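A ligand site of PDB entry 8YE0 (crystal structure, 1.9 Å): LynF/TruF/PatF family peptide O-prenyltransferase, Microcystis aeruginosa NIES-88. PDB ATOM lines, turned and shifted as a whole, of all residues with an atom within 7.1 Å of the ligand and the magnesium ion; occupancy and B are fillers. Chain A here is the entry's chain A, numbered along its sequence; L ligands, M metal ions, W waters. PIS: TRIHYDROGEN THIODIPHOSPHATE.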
ATOM      1  N   LYS A  53     -31.432  18.675 -16.318  1.00  0.00           N
ATOM      2  CA  LYS A  53     -31.175  17.251 -16.465  1.00  0.00           C
ATOM      3  C   LYS A  53     -31.623  16.586 -15.173  1.00  0.00           C
ATOM      4  O   LYS A  53     -31.329  17.077 -14.079  1.00  0.00           O
ATOM      5  CB  LYS A  53     -29.702  16.979 -16.744  1.00  0.00           C
ATOM      6  CG  LYS A  53     -29.199  15.638 -16.243  1.00  0.00           C
ATOM      7  CD  LYS A  53     -27.894  15.226 -16.930  1.00  0.00           C
ATOM      8  CE  LYS A  53     -27.507  13.790 -16.546  1.00  0.00           C
ATOM      9  NZ  LYS A  53     -26.714  13.082 -17.581  1.00  0.00           N
ATOM     10  N   ARG A  63     -28.242  24.572 -16.967  1.00  0.00           N
ATOM     11  CA  ARG A  63     -28.031  24.156 -18.342  1.00  0.00           C
ATOM     12  C   ARG A  63     -28.675  25.168 -19.274  1.00  0.00           C
ATOM     13  O   ARG A  63     -29.876  25.454 -19.156  1.00  0.00           O
ATOM     14  CB  ARG A  63     -28.599  22.758 -18.600  1.00  0.00           C
ATOM     15  CG  ARG A  63     -27.898  21.658 -17.795  1.00  0.00           C
ATOM     16  CD  ARG A  63     -28.419  20.253 -18.168  1.00  0.00           C
ATOM     17  NE  ARG A  63     -28.458  20.030 -19.613  1.00  0.00           N
ATOM     18  CZ  ARG A  63     -27.630  19.230 -20.266  1.00  0.00           C
ATOM     19  NH1 ARG A  63     -26.706  18.520 -19.637  1.00  0.00           N
ATOM     20  NH2 ARG A  63     -27.734  19.134 -21.588  1.00  0.00           N
ATOM     21  N   SER A  65     -28.384  26.783 -23.547  1.00  0.00           N
ATOM     22  CA  SER A  65     -27.812  26.739 -24.884  1.00  0.00           C
ATOM     23  C   SER A  65     -28.203  28.013 -25.617  1.00  0.00           C
ATOM     24  O   SER A  65     -29.329  28.490 -25.481  1.00  0.00           O
ATOM     25  CB  SER A  65     -28.303  25.526 -25.681  1.00  0.00           C
ATOM     26  OG  SER A  65     -28.154  24.333 -24.941  1.00  0.00           O
ATOM     27  N   ASP A 122     -23.274  23.402 -18.770  1.00  0.00           N
ATOM     28  CA  ASP A 122     -23.965  22.571 -17.785  1.00  0.00           C
ATOM     29  C   ASP A 122     -23.089  22.677 -16.543  1.00  0.00           C
ATOM     30  O   ASP A 122     -22.128  21.918 -16.404  1.00  0.00           O
ATOM     31  CB  ASP A 122     -24.142  21.142 -18.261  1.00  0.00           C
ATOM     32  CG  ASP A 122     -24.781  20.229 -17.208  1.00  0.00           C
ATOM     33  OD1 ASP A 122     -24.945  20.638 -16.035  1.00  0.00           O
ATOM     34  OD2 ASP A 122     -25.112  19.081 -17.555  1.00  0.00           O
ATOM     35  N   ARG A 124     -21.989  22.558 -12.641  1.00  0.00           N
ATOM     36  CA  ARG A 124     -22.210  21.593 -11.582  1.00  0.00           C
ATOM     37  C   ARG A 124     -21.615  22.129 -10.283  1.00  0.00           C
ATOM     38  O   ARG A 124     -20.727  22.995 -10.297  1.00  0.00           O
ATOM     39  CB  ARG A 124     -21.576  20.239 -11.930  1.00  0.00           C
ATOM     40  CG  ARG A 124     -22.169  19.579 -13.178  1.00  0.00           C
ATOM     41  CD  ARG A 124     -23.637  19.213 -12.998  1.00  0.00           C
ATOM     42  NE  ARG A 124     -24.185  18.567 -14.182  1.00  0.00           N
ATOM     43  CZ  ARG A 124     -24.096  17.273 -14.452  1.00  0.00           C
ATOM     44  NH1 ARG A 124     -23.497  16.429 -13.626  1.00  0.00           N
ATOM     45  NH2 ARG A 124     -24.641  16.803 -15.579  1.00  0.00           N
ATOM     46  N   ARG A 131     -19.354  21.426 -17.590  1.00  0.00           N
ATOM     47  CA  ARG A 131     -18.990  21.400 -18.998  1.00  0.00           C
ATOM     48  C   ARG A 131     -19.336  22.734 -19.632  1.00  0.00           C
ATOM     49  O   ARG A 131     -20.298  23.389 -19.247  1.00  0.00           O
ATOM     50  CB  ARG A 131     -19.733  20.297 -19.765  1.00  0.00           C
ATOM     51  CG  ARG A 131     -19.227  18.885 -19.520  1.00  0.00           C
ATOM     52  CD  ARG A 131     -20.187  17.884 -20.117  1.00  0.00           C
ATOM     53  NE  ARG A 131     -21.465  17.871 -19.413  1.00  0.00           N
ATOM     54  CZ  ARG A 131     -22.530  17.176 -19.790  1.00  0.00           C
ATOM     55  NH1 ARG A 131     -22.507  16.428 -20.887  1.00  0.00           N
ATOM     56  NH2 ARG A 131     -23.635  17.230 -19.056  1.00  0.00           N
ATOM     57  N   LYS A 133     -19.958  23.623 -23.845  1.00  0.00           N
ATOM     58  CA  LYS A 133     -20.325  22.815 -25.004  1.00  0.00           C
ATOM     59  C   LYS A 133     -20.287  23.656 -26.266  1.00  0.00           C
ATOM     60  O   LYS A 133     -20.674  24.828 -26.235  1.00  0.00           O
ATOM     61  CB  LYS A 133     -21.721  22.214 -24.827  1.00  0.00           C
ATOM     62  CG  LYS A 133     -21.850  21.299 -23.607  1.00  0.00           C
ATOM     63  CD  LYS A 133     -23.306  21.224 -23.122  1.00  0.00           C
ATOM     64  CE  LYS A 133     -23.571  19.905 -22.369  1.00  0.00           C
ATOM     65  NZ  LYS A 133     -23.515  18.712 -23.267  1.00  0.00           N
ATOM     66  N   TYR A 135     -21.727  23.102 -30.294  1.00  0.00           N
ATOM     67  CA  TYR A 135     -22.451  22.307 -31.278  1.00  0.00           C
ATOM     68  C   TYR A 135     -22.334  22.981 -32.637  1.00  0.00           C
ATOM     69  O   TYR A 135     -22.627  24.175 -32.762  1.00  0.00           O
ATOM     70  CB  TYR A 135     -23.945  22.176 -30.949  1.00  0.00           C
ATOM     71  CG  TYR A 135     -24.315  21.760 -29.543  1.00  0.00           C
ATOM     72  CD1 TYR A 135     -24.388  22.686 -28.523  1.00  0.00           C
ATOM     73  CD2 TYR A 135     -24.637  20.433 -29.249  1.00  0.00           C
ATOM     74  CE1 TYR A 135     -24.759  22.330 -27.251  1.00  0.00           C
ATOM     75  CE2 TYR A 135     -25.013  20.057 -27.968  1.00  0.00           C
ATOM     76  CZ  TYR A 135     -25.067  21.008 -26.983  1.00  0.00           C
ATOM     77  OH  TYR A 135     -25.432  20.676 -25.711  1.00  0.00           O
ATOM     78  N   GLY A 170     -21.665  17.634 -31.598  1.00  0.00           N
ATOM     79  CA  GLY A 170     -21.560  18.279 -30.305  1.00  0.00           C
ATOM     80  C   GLY A 170     -20.243  17.925 -29.648  1.00  0.00           C
ATOM     81  O   GLY A 170     -19.822  16.757 -29.665  1.00  0.00           O
ATOM     82  N   ASP A 172     -18.184  18.189 -25.989  1.00  0.00           N
ATOM     83  CA  ASP A 172     -18.240  18.408 -24.548  1.00  0.00           C
ATOM     84  C   ASP A 172     -16.836  18.673 -24.030  1.00  0.00           C
ATOM     85  O   ASP A 172     -15.889  17.971 -24.383  1.00  0.00           O
ATOM     86  CB  ASP A 172     -18.829  17.179 -23.822  1.00  0.00           C
ATOM     87  CG  ASP A 172     -20.344  17.190 -23.778  1.00  0.00           C
ATOM     88  OD1 ASP A 172     -20.950  18.182 -24.226  1.00  0.00           O
ATOM     89  OD2 ASP A 172     -20.925  16.201 -23.272  1.00  0.00           O
ATOM     90  N   TYR A 174     -15.256  18.993 -20.412  1.00  0.00           N
ATOM     91  CA  TYR A 174     -15.292  18.949 -18.953  1.00  0.00           C
ATOM     92  C   TYR A 174     -14.158  19.784 -18.362  1.00  0.00           C
ATOM     93  O   TYR A 174     -13.060  19.854 -18.905  1.00  0.00           O
ATOM     94  CB  TYR A 174     -15.188  17.503 -18.452  1.00  0.00           C
ATOM     95  CG  TYR A 174     -16.406  16.650 -18.671  1.00  0.00           C
ATOM     96  CD1 TYR A 174     -16.572  15.923 -19.843  1.00  0.00           C
ATOM     97  CD2 TYR A 174     -17.392  16.540 -17.693  1.00  0.00           C
ATOM     98  CE1 TYR A 174     -17.689  15.115 -20.044  1.00  0.00           C
ATOM     99  CE2 TYR A 174     -18.510  15.744 -17.887  1.00  0.00           C
ATOM    100  CZ  TYR A 174     -18.648  15.035 -19.061  1.00  0.00           C
ATOM    101  OH  TYR A 174     -19.760  14.238 -19.234  1.00  0.00           O
ATOM    102  N   GLU A 182     -20.301  13.992 -29.944  1.00  0.00           N
ATOM    103  CA  GLU A 182     -21.588  13.351 -30.163  1.00  0.00           C
ATOM    104  C   GLU A 182     -22.123  13.738 -31.535  1.00  0.00           C
ATOM    105  O   GLU A 182     -21.920  14.865 -31.990  1.00  0.00           O
ATOM    106  CB  GLU A 182     -22.597  13.758 -29.076  1.00  0.00           C
ATOM    107  CG  GLU A 182     -23.936  13.025 -29.150  1.00  0.00           C
ATOM    108  CD  GLU A 182     -24.770  13.215 -27.883  1.00  0.00           C
ATOM    109  OE1 GLU A 182     -24.451  14.136 -27.101  1.00  0.00           O
ATOM    110  OE2 GLU A 182     -25.714  12.422 -27.659  1.00  0.00           O
ATOM    111  N   TYR A 184     -25.624  13.956 -33.857  1.00  0.00           N
ATOM    112  CA  TYR A 184     -27.084  13.956 -33.851  1.00  0.00           C
ATOM    113  C   TYR A 184     -27.614  14.143 -35.261  1.00  0.00           C
ATOM    114  O   TYR A 184     -27.153  15.013 -36.004  1.00  0.00           O
ATOM    115  CB  TYR A 184     -27.686  15.071 -32.982  1.00  0.00           C
ATOM    116  CG  TYR A 184     -26.984  15.414 -31.688  1.00  0.00           C
ATOM    117  CD1 TYR A 184     -25.797  16.145 -31.686  1.00  0.00           C
ATOM    118  CD2 TYR A 184     -27.557  15.091 -30.451  1.00  0.00           C
ATOM    119  CE1 TYR A 184     -25.176  16.506 -30.495  1.00  0.00           C
ATOM    120  CE2 TYR A 184     -26.936  15.451 -29.259  1.00  0.00           C
ATOM    121  CZ  TYR A 184     -25.753  16.159 -29.291  1.00  0.00           C
ATOM    122  OH  TYR A 184     -25.136  16.525 -28.112  1.00  0.00           O
ATOM    123  N   GLY A 222     -29.071  11.085 -30.821  1.00  0.00           N
ATOM    124  CA  GLY A 222     -27.672  11.375 -30.564  1.00  0.00           C
ATOM    125  C   GLY A 222     -26.929  10.110 -30.179  1.00  0.00           C
ATOM    126  O   GLY A 222     -27.378   9.342 -29.316  1.00  0.00           O
ATOM    127  N   SER A 224     -22.891   8.598 -29.254  1.00  0.00           N
ATOM    128  CA  SER A 224     -21.596   9.049 -28.750  1.00  0.00           C
ATOM    129  C   SER A 224     -20.949   7.897 -27.991  1.00  0.00           C
ATOM    130  O   SER A 224     -21.643   7.073 -27.403  1.00  0.00           O
ATOM    131  CB  SER A 224     -21.736  10.269 -27.839  1.00  0.00           C
ATOM    132  OG  SER A 224     -20.514  10.569 -27.184  1.00  0.00           O
ATOM    133  N   ALA A 226     -19.632   8.309 -25.307  1.00  0.00           N
ATOM    134  CA  ALA A 226     -19.937   8.628 -23.920  1.00  0.00           C
ATOM    135  C   ALA A 226     -21.374   8.316 -23.526  1.00  0.00           C
ATOM    136  O   ALA A 226     -21.723   8.466 -22.358  1.00  0.00           O
ATOM    137  CB  ALA A 226     -19.652  10.110 -23.648  1.00  0.00           C
ATOM    138  N   ASN A 227     -22.210   7.910 -24.477  1.00  0.00           N
ATOM    139  CA  ASN A 227     -23.594   7.559 -24.196  1.00  0.00           C
ATOM    140  C   ASN A 227     -23.701   6.094 -23.804  1.00  0.00           C
ATOM    141  O   ASN A 227     -23.074   5.229 -24.430  1.00  0.00           O
ATOM    142  CB  ASN A 227     -24.481   7.844 -25.412  1.00  0.00           C
ATOM    143  CG  ASN A 227     -24.634   9.335 -25.694  1.00  0.00           C
ATOM    144  OD1 ASN A 227     -24.260  10.173 -24.877  1.00  0.00           O
ATOM    145  ND2 ASN A 227     -25.173   9.662 -26.865  1.00  0.00           N
ATOM    146  N   ILE A 231     -29.561   8.376 -27.476  1.00  0.00           N
ATOM    147  CA  ILE A 231     -30.368   9.390 -26.794  1.00  0.00           C
ATOM    148  C   ILE A 231     -31.423   9.879 -27.780  1.00  0.00           C
ATOM    149  O   ILE A 231     -31.085  10.411 -28.845  1.00  0.00           O
ATOM    150  CB  ILE A 231     -29.497  10.545 -26.279  1.00  0.00           C
ATOM    151  CG1 ILE A 231     -28.337  10.029 -25.441  1.00  0.00           C
ATOM    152  CG2 ILE A 231     -30.348  11.494 -25.442  1.00  0.00           C
ATOM    153  CD1 ILE A 231     -28.753   9.317 -24.180  1.00  0.00           C
ATOM    154  N   TYR A 233     -34.303  12.459 -28.750  1.00  0.00           N
ATOM    155  CA  TYR A 233     -34.724  13.834 -28.501  1.00  0.00           C
ATOM    156  C   TYR A 233     -36.124  13.998 -29.077  1.00  0.00           C
ATOM    157  O   TYR A 233     -36.312  13.983 -30.297  1.00  0.00           O
ATOM    158  CB  TYR A 233     -33.757  14.838 -29.123  1.00  0.00           C
ATOM    159  CG  TYR A 233     -32.431  14.908 -28.423  1.00  0.00           C
ATOM    160  CD1 TYR A 233     -31.489  13.902 -28.584  1.00  0.00           C
ATOM    161  CD2 TYR A 233     -32.125  15.954 -27.560  1.00  0.00           C
ATOM    162  CE1 TYR A 233     -30.266  13.948 -27.934  1.00  0.00           C
ATOM    163  CE2 TYR A 233     -30.899  16.004 -26.901  1.00  0.00           C
ATOM    164  CZ  TYR A 233     -29.974  14.994 -27.090  1.00  0.00           C
ATOM    165  OH  TYR A 233     -28.762  15.035 -26.447  1.00  0.00           O
ATOM    166  N   CYS A 269     -35.390  14.730 -23.908  1.00  0.00           N
ATOM    167  CA  CYS A 269     -34.517  13.676 -24.388  1.00  0.00           C
ATOM    168  C   CYS A 269     -34.414  12.587 -23.332  1.00  0.00           C
ATOM    169  O   CYS A 269     -34.349  12.859 -22.131  1.00  0.00           O
ATOM    170  CB  CYS A 269     -33.123  14.190 -24.770  1.00  0.00           C
ATOM    171  SG  CYS A 269     -31.944  14.232 -23.443  1.00  0.00           S
ATOM    172  N   LEU A 283     -33.523  11.944 -17.777  1.00  0.00           N
ATOM    173  CA  LEU A 283     -34.082  12.673 -18.914  1.00  0.00           C
ATOM    174  C   LEU A 283     -33.610  14.110 -18.809  1.00  0.00           C
ATOM    175  O   LEU A 283     -33.278  14.595 -17.729  1.00  0.00           O
ATOM    176  CB  LEU A 283     -35.609  12.603 -18.933  1.00  0.00           C
ATOM    177  CG  LEU A 283     -36.352  13.323 -17.812  1.00  0.00           C
ATOM    178  CD1 LEU A 283     -37.594  14.016 -18.347  1.00  0.00           C
ATOM    179  CD2 LEU A 283     -36.735  12.346 -16.699  1.00  0.00           C
ATOM    180  N   ASN A 284     -33.580  14.780 -19.966  1.00  0.00           N
ATOM    181  CA  ASN A 284     -33.354  16.216 -20.015  1.00  0.00           C
ATOM    182  C   ASN A 284     -34.600  16.884 -20.584  1.00  0.00           C
ATOM    183  O   ASN A 284     -35.284  16.319 -21.450  1.00  0.00           O
ATOM    184  CB  ASN A 284     -32.133  16.571 -20.883  1.00  0.00           C
ATOM    185  CG  ASN A 284     -30.846  15.976 -20.352  1.00  0.00           C
ATOM    186  OD1 ASN A 284     -30.804  15.402 -19.257  1.00  0.00           O
ATOM    187  ND2 ASN A 284     -29.774  16.105 -21.133  1.00  0.00           N
ATOM    188  N   TYR A 286     -35.615  20.536 -22.344  1.00  0.00           N
ATOM    189  CA  TYR A 286     -35.108  21.773 -22.928  1.00  0.00           C
ATOM    190  C   TYR A 286     -36.290  22.655 -23.289  1.00  0.00           C
ATOM    191  O   TYR A 286     -37.145  22.254 -24.096  1.00  0.00           O
ATOM    192  CB  TYR A 286     -34.252  21.526 -24.186  1.00  0.00           C
ATOM    193  CG  TYR A 286     -33.198  20.459 -24.056  1.00  0.00           C
ATOM    194  CD1 TYR A 286     -33.546  19.107 -24.108  1.00  0.00           C
ATOM    195  CD2 TYR A 286     -31.863  20.791 -23.905  1.00  0.00           C
ATOM    196  CE1 TYR A 286     -32.583  18.119 -23.995  1.00  0.00           C
ATOM    197  CE2 TYR A 286     -30.888  19.808 -23.785  1.00  0.00           C
ATOM    198  CZ  TYR A 286     -31.252  18.473 -23.841  1.00  0.00           C
ATOM    199  OH  TYR A 286     -30.300  17.480 -23.735  1.00  0.00           O
HETATM  200  P1  PIS L   1     -26.757  17.158 -24.771  1.00  0.00           P
HETATM  201  O1  PIS L   1     -26.973  16.528 -23.314  1.00  0.00           O
HETATM  202  P2  PIS L   1     -26.052  15.690 -22.315  1.00  0.00           P
HETATM  203  S1  PIS L   1     -27.232  14.836 -21.040  1.00  0.00           S
HETATM  204  O2  PIS L   1     -28.155  17.423 -25.224  1.00  0.00           O
HETATM  205  O3  PIS L   1     -25.945  18.428 -24.589  1.00  0.00           O
HETATM  206  O4  PIS L   1     -25.288  14.790 -23.222  1.00  0.00           O
HETATM  207  O5  PIS L   1     -26.044  16.145 -25.623  1.00  0.00           O
HETATM  208  O6  PIS L   1     -25.118  16.714 -21.723  1.00  0.00           O
HETATM  209 MG    MG M   1     -24.897  14.510 -25.133  1.00  0.00          MG
HETATM  210  O   HOH W   1     -23.780  12.714 -24.582  1.00  0.00           O
HETATM  211  O   HOH W   2     -23.197  15.561 -25.021  1.00  0.00           O
HETATM  212  O   HOH W   3     -26.751  13.308 -25.517  1.00  0.00           O
HETATM  213  O   HOH W   4     -23.270  13.231 -21.750  1.00  0.00           O
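OH of Tyr 135 is in hydrogen-bond range of O3 of the ligand (2.6 Å).
The side-chain hydroxyl (OH) of Tyr 286 lies within hydrogen-bond range of an oxygen (O2) of the ligand (2.6 Å).
The side-chain hydroxyl (OH) of Tyr 184 sits close to an oxygen (O5) of the ligand, 2.7 Å away.
OH of Tyr 233 lies within hydrogen-bond range of O2 of the ligand (2.8 Å).
The guanidinium group of Arg 131 is in salt-bridge range of an oxygen (O6) of the ligand (2.8 Å).
O3 of the ligand is in salt-bridge range of NZ of Lys 133.
ND2 of Asn 284 sits close to S1 of the ligand, 2.8 Å away.
The guanidinium group of Arg 63 lies within salt-bridge range of an oxygen (O6) of the ligand (3.2 Å).
The side-chain carboxylate of Glu 182 sits close to the side-chain hydroxyl of Tyr 184 (2.7 Å).
The side-chain amide nitrogen (ND2) of Asn 227 lies within hydrogen-bond range of the side-chain carboxylate (OE2) of Glu 182, at 2.9 Å.
The backbone NH of Gly 170 lies within hydrogen-bond range of the backbone carbonyl oxygen of Glu 182.
OH of Tyr 286 sits at hydrogen-bond distance from SG of Cys 269.
NH1 of Arg 131 lies within salt-bridge range of OD2 of Asp 172, 2.9 Å away.
The side-chain carboxylate (OD2) of Asp 122 is in salt-bridge range of the guanidinium group (NH2) of Arg 131, 2.8 Å away.
The backbone NH of Cys 269 is in hydrogen-bond range of the backbone carbonyl oxygen of Asn 284 (2.9 Å).
The guanidinium group of Arg 63 is in salt-bridge range of the side-chain carboxylate of Asp 122.
Lys 53 touches the ligand (NZ to S1, 3.9 Å).
Hydrophobic or aromatic side chains within 4 Å of the ligand: Tyr 135, Tyr 184, Tyr 233 and Tyr 286.
The nearest printed residue that does not touch the ligand is Asp 172 (4.5 Å).
Residues that only touch the magnesium ion: Tyr 184 (3.6 Å).
Of the 23 residues printed, 2 come within 4 Å of the magnesium ion.
An oxygen (O4) of the ligand binds the magnesium ion (2.0 Å).
Water W2 binds the magnesium ion (2.0 Å).
OE1 of Glu 182 binds the magnesium ion.
O5 of the ligand binds the magnesium ion, at 2.1 Å.
Water W1 is bound to the magnesium ion (2.2 Å).
The magnesium ion is bound by water W3, 2.2 Å away.
The magnesium ion has six donor atoms within binding distance.
Water W3 lies within hydrogen-bond range of the side-chain carboxylate (OE2) of Glu 182 (2.5 Å) and the side-chain hydroxyl (OH) of Tyr 233 (2.8 Å).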
